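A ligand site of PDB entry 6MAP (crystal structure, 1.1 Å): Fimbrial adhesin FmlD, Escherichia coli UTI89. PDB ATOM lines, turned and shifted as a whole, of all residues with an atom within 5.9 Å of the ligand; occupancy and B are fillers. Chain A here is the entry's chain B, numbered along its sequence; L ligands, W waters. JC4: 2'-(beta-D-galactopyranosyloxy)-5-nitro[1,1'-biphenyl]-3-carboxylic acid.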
ATOM      1  N   PHE A   1       6.919  -5.168  -5.146  1.00  0.00           N
ATOM      2  CA  PHE A   1       7.834  -5.040  -6.287  1.00  0.00           C
ATOM      3  C   PHE A   1       7.337  -5.951  -7.403  1.00  0.00           C
ATOM      4  O   PHE A   1       6.955  -7.081  -7.129  1.00  0.00           O
ATOM      5  CB  PHE A   1       9.250  -5.438  -5.897  1.00  0.00           C
ATOM      6  CG  PHE A   1      10.219  -5.428  -7.051  1.00  0.00           C
ATOM      7  CD1 PHE A   1      10.609  -6.616  -7.656  1.00  0.00           C
ATOM      8  CD2 PHE A   1      10.721  -4.242  -7.534  1.00  0.00           C
ATOM      9  CE1 PHE A   1      11.488  -6.613  -8.732  1.00  0.00           C
ATOM     10  CE2 PHE A   1      11.595  -4.232  -8.599  1.00  0.00           C
ATOM     11  CZ  PHE A   1      11.985  -5.422  -9.194  1.00  0.00           C
ATOM     12  N   SER A   2       7.351  -5.463  -8.637  1.00  0.00           N
ATOM     13  CA  SER A   2       6.853  -6.254  -9.757  1.00  0.00           C
ATOM     14  C   SER A   2       7.602  -5.924 -11.023  1.00  0.00           C
ATOM     15  O   SER A   2       8.144  -4.835 -11.167  1.00  0.00           O
ATOM     16  CB  SER A   2       5.378  -5.937 -10.023  1.00  0.00           C
ATOM     17  OG  SER A   2       4.536  -6.141  -8.907  1.00  0.00           O
ATOM     18  N   CYS A   3       7.567  -6.867 -11.967  1.00  0.00           N
ATOM     19  CA  CYS A   3       8.122  -6.666 -13.287  1.00  0.00           C
ATOM     20  C   CYS A   3       7.147  -7.165 -14.329  1.00  0.00           C
ATOM     21  O   CYS A   3       6.214  -7.904 -14.019  1.00  0.00           O
ATOM     22  CB  CYS A   3       9.407  -7.483 -13.434  1.00  0.00           C
ATOM     23  SG  CYS A   3      10.681  -7.123 -12.218  1.00  0.00           S
ATOM     24  N   SER A  10       1.996  -8.982 -14.596  1.00  0.00           N
ATOM     25  CA  SER A  10       2.947  -8.620 -13.565  1.00  0.00           C
ATOM     26  C   SER A  10       3.555  -9.852 -12.912  1.00  0.00           C
ATOM     27  O   SER A  10       2.890 -10.874 -12.737  1.00  0.00           O
ATOM     28  CB  SER A  10       2.259  -7.746 -12.526  1.00  0.00           C
ATOM     29  OG  SER A  10       1.813  -6.556 -13.152  1.00  0.00           O
ATOM     30  N   ILE A  11       4.837  -9.743 -12.581  1.00  0.00           N
ATOM     31  CA  ILE A  11       5.625 -10.861 -12.092  1.00  0.00           C
ATOM     32  C   ILE A  11       6.308 -10.428 -10.798  1.00  0.00           C
ATOM     33  O   ILE A  11       7.049  -9.437 -10.783  1.00  0.00           O
ATOM     34  CB  ILE A  11       6.728 -11.231 -13.110  1.00  0.00           C
ATOM     35  CG1 ILE A  11       6.126 -11.506 -14.490  1.00  0.00           C
ATOM     36  CG2 ILE A  11       7.530 -12.423 -12.606  1.00  0.00           C
ATOM     37  CD1 ILE A  11       7.165 -11.434 -15.607  1.00  0.00           C
ATOM     38  N   GLY A  12       6.086 -11.179  -9.730  1.00  0.00           N
ATOM     39  CA  GLY A  12       6.652 -10.835  -8.438  1.00  0.00           C
ATOM     40  C   GLY A  12       7.737 -11.787  -7.986  1.00  0.00           C
ATOM     41  O   GLY A  12       8.437 -11.513  -7.002  1.00  0.00           O
ATOM     42  N   ALA A  13       7.891 -12.912  -8.697  1.00  0.00           N
ATOM     43  CA  ALA A  13       8.882 -13.918  -8.372  1.00  0.00           C
ATOM     44  C   ALA A  13       8.776 -14.986  -9.427  1.00  0.00           C
ATOM     45  O   ALA A  13       7.832 -15.002 -10.209  1.00  0.00           O
ATOM     46  CB  ALA A  13       8.613 -14.541  -7.011  1.00  0.00           C
ATOM     47  N   TRP A  43       9.082  -2.158 -11.291  1.00  0.00           N
ATOM     48  CA  TRP A  43       8.678  -0.966 -10.573  1.00  0.00           C
ATOM     49  C   TRP A  43       8.407  -1.314  -9.122  1.00  0.00           C
ATOM     50  O   TRP A  43       8.238  -2.471  -8.744  1.00  0.00           O
ATOM     51  CB  TRP A  43       7.414  -0.353 -11.197  1.00  0.00           C
ATOM     52  CG  TRP A  43       6.263  -1.302 -11.227  1.00  0.00           C
ATOM     53  CD1 TRP A  43       5.303  -1.452 -10.277  1.00  0.00           C
ATOM     54  CD2 TRP A  43       5.979  -2.273 -12.236  1.00  0.00           C
ATOM     55  NE1 TRP A  43       4.420  -2.449 -10.636  1.00  0.00           N
ATOM     56  CE2 TRP A  43       4.819  -2.976 -11.833  1.00  0.00           C
ATOM     57  CE3 TRP A  43       6.595  -2.627 -13.450  1.00  0.00           C
ATOM     58  CZ2 TRP A  43       4.261  -4.003 -12.608  1.00  0.00           C
ATOM     59  CZ3 TRP A  43       6.036  -3.658 -14.205  1.00  0.00           C
ATOM     60  CH2 TRP A  43       4.885  -4.326 -13.795  1.00  0.00           C
ATOM     61  N   ASN A  44       8.383  -0.258  -8.308  1.00  0.00           N
ATOM     62  CA  ASN A  44       7.983  -0.348  -6.918  1.00  0.00           C
ATOM     63  C   ASN A  44       6.463  -0.216  -6.847  1.00  0.00           C
ATOM     64  O   ASN A  44       5.881   0.628  -7.531  1.00  0.00           O
ATOM     65  CB  ASN A  44       8.710   0.779  -6.157  1.00  0.00           C
ATOM     66  CG  ASN A  44       8.255   0.940  -4.713  1.00  0.00           C
ATOM     67  OD1 ASN A  44       7.125   1.324  -4.451  1.00  0.00           O
ATOM     68  ND2 ASN A  44       9.170   0.697  -3.784  1.00  0.00           N
ATOM     69  N   ASP A  45       5.824  -1.062  -6.048  1.00  0.00           N
ATOM     70  CA  ASP A  45       4.368  -1.138  -6.071  1.00  0.00           C
ATOM     71  C   ASP A  45       3.663  -0.058  -5.265  1.00  0.00           C
ATOM     72  O   ASP A  45       2.434   0.090  -5.365  1.00  0.00           O
ATOM     73  CB  ASP A  45       3.904  -2.524  -5.662  1.00  0.00           C
ATOM     74  CG  ASP A  45       3.979  -3.503  -6.804  1.00  0.00           C
ATOM     75  OD1 ASP A  45       3.311  -3.235  -7.822  1.00  0.00           O
ATOM     76  OD2 ASP A  45       4.740  -4.485  -6.707  1.00  0.00           O
ATOM     77  N   TYR A  46       4.419   0.719  -4.498  1.00  0.00           N
ATOM     78  CA  TYR A  46       3.864   1.848  -3.758  1.00  0.00           C
ATOM     79  C   TYR A  46       4.117   3.173  -4.474  1.00  0.00           C
ATOM     80  O   TYR A  46       3.280   4.084  -4.426  1.00  0.00           O
ATOM     81  CB  TYR A  46       4.468   1.934  -2.357  1.00  0.00           C
ATOM     82  CG  TYR A  46       4.179   0.746  -1.468  1.00  0.00           C
ATOM     83  CD1 TYR A  46       2.902   0.222  -1.358  1.00  0.00           C
ATOM     84  CD2 TYR A  46       5.203   0.170  -0.731  1.00  0.00           C
ATOM     85  CE1 TYR A  46       2.656  -0.860  -0.537  1.00  0.00           C
ATOM     86  CE2 TYR A  46       4.972  -0.895   0.094  1.00  0.00           C
ATOM     87  CZ  TYR A  46       3.701  -1.405   0.198  1.00  0.00           C
ATOM     88  OH  TYR A  46       3.487  -2.485   1.020  1.00  0.00           O
ATOM     89  N   TYR A  50       8.727   4.699  -1.472  1.00  0.00           N
ATOM     90  CA  TYR A  50       8.267   4.134  -0.218  1.00  0.00           C
ATOM     91  C   TYR A  50       8.573   2.637  -0.217  1.00  0.00           C
ATOM     92  O   TYR A  50       8.163   1.925  -1.133  1.00  0.00           O
ATOM     93  CB  TYR A  50       6.767   4.380  -0.029  1.00  0.00           C
ATOM     94  CG  TYR A  50       6.346   4.103   1.382  1.00  0.00           C
ATOM     95  CD1 TYR A  50       6.427   5.094   2.338  1.00  0.00           C
ATOM     96  CD2 TYR A  50       5.914   2.843   1.769  1.00  0.00           C
ATOM     97  CE1 TYR A  50       6.076   4.866   3.639  1.00  0.00           C
ATOM     98  CE2 TYR A  50       5.556   2.596   3.096  1.00  0.00           C
ATOM     99  CZ  TYR A  50       5.650   3.621   4.019  1.00  0.00           C
ATOM    100  OH  TYR A  50       5.294   3.400   5.331  1.00  0.00           O
ATOM    101  N   ASP A  51       9.288   2.178   0.803  1.00  0.00           N
ATOM    102  CA  ASP A  51       9.744   0.784   0.851  1.00  0.00           C
ATOM    103  C   ASP A  51      10.536   0.431  -0.408  1.00  0.00           C
ATOM    104  O   ASP A  51      10.176  -0.466  -1.178  1.00  0.00           O
ATOM    105  CB  ASP A  51       8.578  -0.167   1.067  1.00  0.00           C
ATOM    106  CG  ASP A  51       9.007  -1.522   1.615  1.00  0.00           C
ATOM    107  OD1 ASP A  51      10.197  -1.683   1.916  1.00  0.00           O
ATOM    108  OD2 ASP A  51       8.133  -2.397   1.744  1.00  0.00           O
ATOM    109  N   THR A  52      11.620   1.160  -0.603  1.00  0.00           N
ATOM    110  CA  THR A  52      12.418   1.039  -1.811  1.00  0.00           C
ATOM    111  C   THR A  52      12.932  -0.382  -2.002  1.00  0.00           C
ATOM    112  O   THR A  52      13.350  -1.057  -1.070  1.00  0.00           O
ATOM    113  CB  THR A  52      13.571   2.045  -1.790  1.00  0.00           C
ATOM    114  OG1 THR A  52      13.042   3.388  -1.883  1.00  0.00           O
ATOM    115  CG2 THR A  52      14.488   1.821  -2.966  1.00  0.00           C
ATOM    116  N   ASP A  53      12.878  -0.824  -3.247  1.00  0.00           N
ATOM    117  CA  ASP A  53      13.299  -2.164  -3.638  1.00  0.00           C
ATOM    118  C   ASP A  53      14.759  -2.176  -4.033  1.00  0.00           C
ATOM    119  O   ASP A  53      15.237  -1.257  -4.688  1.00  0.00           O
ATOM    120  CB  ASP A  53      12.409  -2.631  -4.783  1.00  0.00           C
ATOM    121  CG  ASP A  53      10.971  -2.781  -4.350  1.00  0.00           C
ATOM    122  OD1 ASP A  53      10.760  -3.622  -3.465  1.00  0.00           O
ATOM    123  OD2 ASP A  53      10.096  -2.060  -4.877  1.00  0.00           O
ATOM    124  N   ILE A  94      14.963   0.647  -6.770  1.00  0.00           N
ATOM    125  CA  ILE A  94      13.755   0.940  -7.534  1.00  0.00           C
ATOM    126  C   ILE A  94      12.674   1.422  -6.594  1.00  0.00           C
ATOM    127  O   ILE A  94      12.324   0.760  -5.623  1.00  0.00           O
ATOM    128  CB  ILE A  94      13.319  -0.295  -8.340  1.00  0.00           C
ATOM    129  CG1 ILE A  94      14.333  -0.536  -9.465  1.00  0.00           C
ATOM    130  CG2 ILE A  94      11.914  -0.106  -8.918  1.00  0.00           C
ATOM    131  CD1 ILE A  94      14.066  -1.748 -10.332  1.00  0.00           C
ATOM    132  N   LYS A 132      15.464  -9.734  -5.217  1.00  0.00           N
ATOM    133  CA  LYS A 132      14.843  -8.524  -4.728  1.00  0.00           C
ATOM    134  C   LYS A 132      14.700  -8.596  -3.212  1.00  0.00           C
ATOM    135  O   LYS A 132      14.258  -9.606  -2.679  1.00  0.00           O
ATOM    136  CB  LYS A 132      13.460  -8.350  -5.350  1.00  0.00           C
ATOM    137  CG  LYS A 132      12.586  -7.300  -4.658  1.00  0.00           C
ATOM    138  CD  LYS A 132      11.552  -7.925  -3.712  1.00  0.00           C
ATOM    139  CE  LYS A 132      10.917  -6.859  -2.814  1.00  0.00           C
ATOM    140  NZ  LYS A 132       9.776  -7.405  -2.028  1.00  0.00           N
ATOM    141  N   ALA A 134      13.313  -5.530  -0.234  1.00  0.00           N
ATOM    142  CA  ALA A 134      12.936  -4.134  -0.034  1.00  0.00           C
ATOM    143  C   ALA A 134      13.523  -3.585   1.261  1.00  0.00           C
ATOM    144  O   ALA A 134      14.571  -4.049   1.707  1.00  0.00           O
ATOM    145  CB  ALA A 134      11.423  -3.984  -0.092  1.00  0.00           C
ATOM    146  N   LEU A 136      11.503  -2.128   4.299  1.00  0.00           N
ATOM    147  CA  LEU A 136      10.766  -2.189   5.551  1.00  0.00           C
ATOM    148  C   LEU A 136      10.493  -3.633   5.965  1.00  0.00           C
ATOM    149  O   LEU A 136      10.329  -4.516   5.122  1.00  0.00           O
ATOM    150  CB  LEU A 136       9.449  -1.437   5.427  1.00  0.00           C
ATOM    151  CG  LEU A 136       9.590   0.041   5.026  1.00  0.00           C
ATOM    152  CD1 LEU A 136       8.212   0.681   4.855  1.00  0.00           C
ATOM    153  CD2 LEU A 136      10.412   0.788   6.066  1.00  0.00           C
ATOM    154  N   GLY A 139      11.583  -7.049   4.293  1.00  0.00           N
ATOM    155  CA  GLY A 139      11.908  -6.696   2.917  1.00  0.00           C
ATOM    156  C   GLY A 139      11.281  -7.634   1.903  1.00  0.00           C
ATOM    157  O   GLY A 139      11.435  -7.426   0.704  1.00  0.00           O
ATOM    158  N   ASN A 140      10.581  -8.656   2.384  1.00  0.00           N
ATOM    159  CA  ASN A 140       9.920  -9.637   1.514  1.00  0.00           C
ATOM    160  C   ASN A 140      10.792 -10.084   0.329  1.00  0.00           C
ATOM    161  O   ASN A 140      10.475  -9.823  -0.843  1.00  0.00           O
ATOM    162  CB  ASN A 140       8.575  -9.105   1.023  1.00  0.00           C
ATOM    163  CG  ASN A 140       7.581  -8.921   2.147  1.00  0.00           C
ATOM    164  OD1 ASN A 140       7.613  -9.668   3.132  1.00  0.00           O
ATOM    165  ND2 ASN A 140       6.707  -7.942   2.014  1.00  0.00           N
ATOM    166  N   ARG A 142      12.503 -11.862  -2.737  1.00  0.00           N
ATOM    167  CA  ARG A 142      11.924 -12.608  -3.850  1.00  0.00           C
ATOM    168  C   ARG A 142      13.032 -13.010  -4.813  1.00  0.00           C
ATOM    169  O   ARG A 142      13.971 -12.254  -5.037  1.00  0.00           O
ATOM    170  CB  ARG A 142      10.898 -11.760  -4.590  1.00  0.00           C
ATOM    171  CG  ARG A 142       9.724 -11.314  -3.752  1.00  0.00           C
ATOM    172  CD  ARG A 142       8.773 -12.468  -3.472  1.00  0.00           C
ATOM    173  NE  ARG A 142       7.603 -12.038  -2.710  1.00  0.00           N
ATOM    174  CZ  ARG A 142       7.472 -12.141  -1.395  1.00  0.00           C
ATOM    175  NH1 ARG A 142       8.444 -12.660  -0.657  1.00  0.00           N
ATOM    176  NH2 ARG A 142       6.362 -11.709  -0.794  1.00  0.00           N
HETATM  177  C10 JC4 L   1       0.771  -4.032  -4.127  1.00  0.00           C
HETATM  178  C13 JC4 L   1       3.082  -6.938  -4.879  1.00  0.00           C
HETATM  179  C15 JC4 L   1       4.276  -9.041  -4.838  1.00  0.00           C
HETATM  180  C20 JC4 L   1       3.287  -8.284  -6.866  1.00  0.00           C
HETATM  181  C24 JC4 L   1       2.821  -7.134  -6.221  1.00  0.00           C
HETATM  182  O01 JC4 L   1       7.607  -2.435  -4.262  1.00  0.00           O
HETATM  183  C02 JC4 L   1       7.340  -1.927  -2.931  1.00  0.00           C
HETATM  184  C03 JC4 L   1       6.850  -3.013  -2.016  1.00  0.00           C
HETATM  185  O04 JC4 L   1       5.832  -3.792  -2.731  1.00  0.00           O
HETATM  186  C05 JC4 L   1       5.177  -4.785  -1.884  1.00  0.00           C
HETATM  187  O06 JC4 L   1       4.420  -5.570  -2.715  1.00  0.00           O
HETATM  188  C07 JC4 L   1       3.202  -5.017  -3.176  1.00  0.00           C
HETATM  189  C08 JC4 L   1       2.638  -3.867  -2.606  1.00  0.00           C
HETATM  190  C09 JC4 L   1       1.432  -3.370  -3.090  1.00  0.00           C
HETATM  191  C11 JC4 L   1       1.323  -5.178  -4.686  1.00  0.00           C
HETATM  192  C12 JC4 L   1       2.538  -5.670  -4.211  1.00  0.00           C
HETATM  193  C14 JC4 L   1       3.800  -7.896  -4.184  1.00  0.00           C
HETATM  194  C16 JC4 L   1       5.082 -10.089  -4.067  1.00  0.00           C
HETATM  195  O17 JC4 L   1       5.223 -11.241  -4.569  1.00  0.00           O
HETATM  196  O18 JC4 L   1       5.589  -9.796  -2.952  1.00  0.00           O
HETATM  197  C19 JC4 L   1       4.015  -9.236  -6.179  1.00  0.00           C
HETATM  198  N21 JC4 L   1       3.002  -8.462  -8.235  1.00  0.00           N
HETATM  199  O22 JC4 L   1       3.691  -9.386  -8.926  1.00  0.00           O
HETATM  200  O23 JC4 L   1       2.120  -7.804  -8.786  1.00  0.00           O
HETATM  201  C25 JC4 L   1       6.189  -5.689  -1.218  1.00  0.00           C
HETATM  202  O26 JC4 L   1       5.491  -6.486  -0.237  1.00  0.00           O
HETATM  203  C27 JC4 L   1       7.285  -4.936  -0.547  1.00  0.00           C
HETATM  204  O28 JC4 L   1       8.285  -5.877  -0.044  1.00  0.00           O
HETATM  205  C29 JC4 L   1       7.912  -3.960  -1.471  1.00  0.00           C
HETATM  206  O30 JC4 L   1       8.550  -4.682  -2.550  1.00  0.00           O
HETATM  207  O   HOH W   1       1.978  -5.115  -9.238  1.00  0.00           O
HETATM  208  O   HOH W   2       4.187  -8.818  -0.829  1.00  0.00           O
HETATM  209  O   HOH W   3       8.935  -4.868   2.368  1.00  0.00           O
HETATM  210  O   HOH W   4      -0.393  -5.692  -7.680  1.00  0.00           O
HETATM  211  O   HOH W   5       7.538  -7.902  -3.746  1.00  0.00           O
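The guanidinium group (NH2) of Arg 142 is in salt-bridge range of an oxygen (O18) of the ligand, at 3.0 Å.
The backbone NH (N) of Gly 12 lies within hydrogen-bond range of an oxygen (O22) of the ligand, at 3.1 Å.
The side-chain amide nitrogen of Asn 140 sits at hydrogen-bond distance from an oxygen (O26) of the ligand (2.9 Å).
N of Asp 45 lies within hydrogen-bond range of O01 of the ligand, at 2.9 Å.
The side-chain carboxylate (OD2) of Asp 53 sits at hydrogen-bond distance from an oxygen (O01) of the ligand.
O28 of the ligand is in hydrogen-bond range of NZ of Lys 132 (2.9 Å).
An oxygen (O23) of the ligand lies within hydrogen-bond range of the side-chain hydroxyl of Ser 2 (2.9 Å).
The backbone NH (N) of Phe 1 is in hydrogen-bond range of an oxygen (O01) of the ligand, 3.0 Å away.
The side-chain hydroxyl (OG) of Ser 2 lies within hydrogen-bond range of the side-chain carboxylate (OD2) of Asp 45 (2.8 Å).
OD1 of Asp 45 is in hydrogen-bond range of NE1 of Trp 43 (3.1 Å).
The backbone carbonyl oxygen of Ser 2 lies within hydrogen-bond range of the backbone NH of Trp 43.
O of Asp 53 sits at hydrogen-bond distance from N of Ile 94, at 2.8 Å.
The backbone NH (N) of Ala 134 sits at hydrogen-bond distance from the backbone carbonyl oxygen (O) of Gly 139, 2.8 Å away.
NH1 of Arg 142 sits close to O of Asn 140, 3.5 Å away.
The side-chain amide nitrogen (ND2) of Asn 44 is in hydrogen-bond range of the backbone carbonyl oxygen (O) of Tyr 50.
OD2 of Asp 53 is in hydrogen-bond range of ND2 of Asn 44, 3.1 Å away.
Ser 10 touches the ligand (CB to O23, 3.7 Å).
C of Ile 11 touches O22 of the ligand (3.4 Å).
Asn 44 touches the ligand.
CE2 of Tyr 46 touches C03 of the ligand, at 3.5 Å.
Asp 51 touches the ligand (OD2 to C27, 3.5 Å).
Ala 134 touches the ligand.
O of Gly 139 touches O28 of the ligand, at 3.6 Å.
Hydrophobic or aromatic side chains that line the ligand: Phe 1, Tyr 46 and Ala 134.
15 residues have an atom within 4 Å of the ligand: Phe 1, Ser 2, Ser 10, Ile 11, Gly 12, Asn 44, Asp 45, Tyr 46, Asp 51, Asp 53, Lys 132, Ala 134, Gly 139, Asn 140 and Arg 142.
Along chain A the residues within 4 Å of the ligand span positions 1 to 142.
Water W3 lies within hydrogen-bond range of the side-chain carboxylate of Asp 51 (2.7 Å), an oxygen (O28) of the ligand (2.7 Å) and the backbone carbonyl oxygen of Leu 136 (3.1 Å).
Water W1 lies within hydrogen-bond range of the side-chain carboxylate (OD1) of Asp 45, an oxygen (O23) of the ligand and the side-chain hydroxyl (OG) of Ser 2.
Water W5 lies within hydrogen-bond range of O18 of the ligand, NZ of Lys 132 and N of Phe 1.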
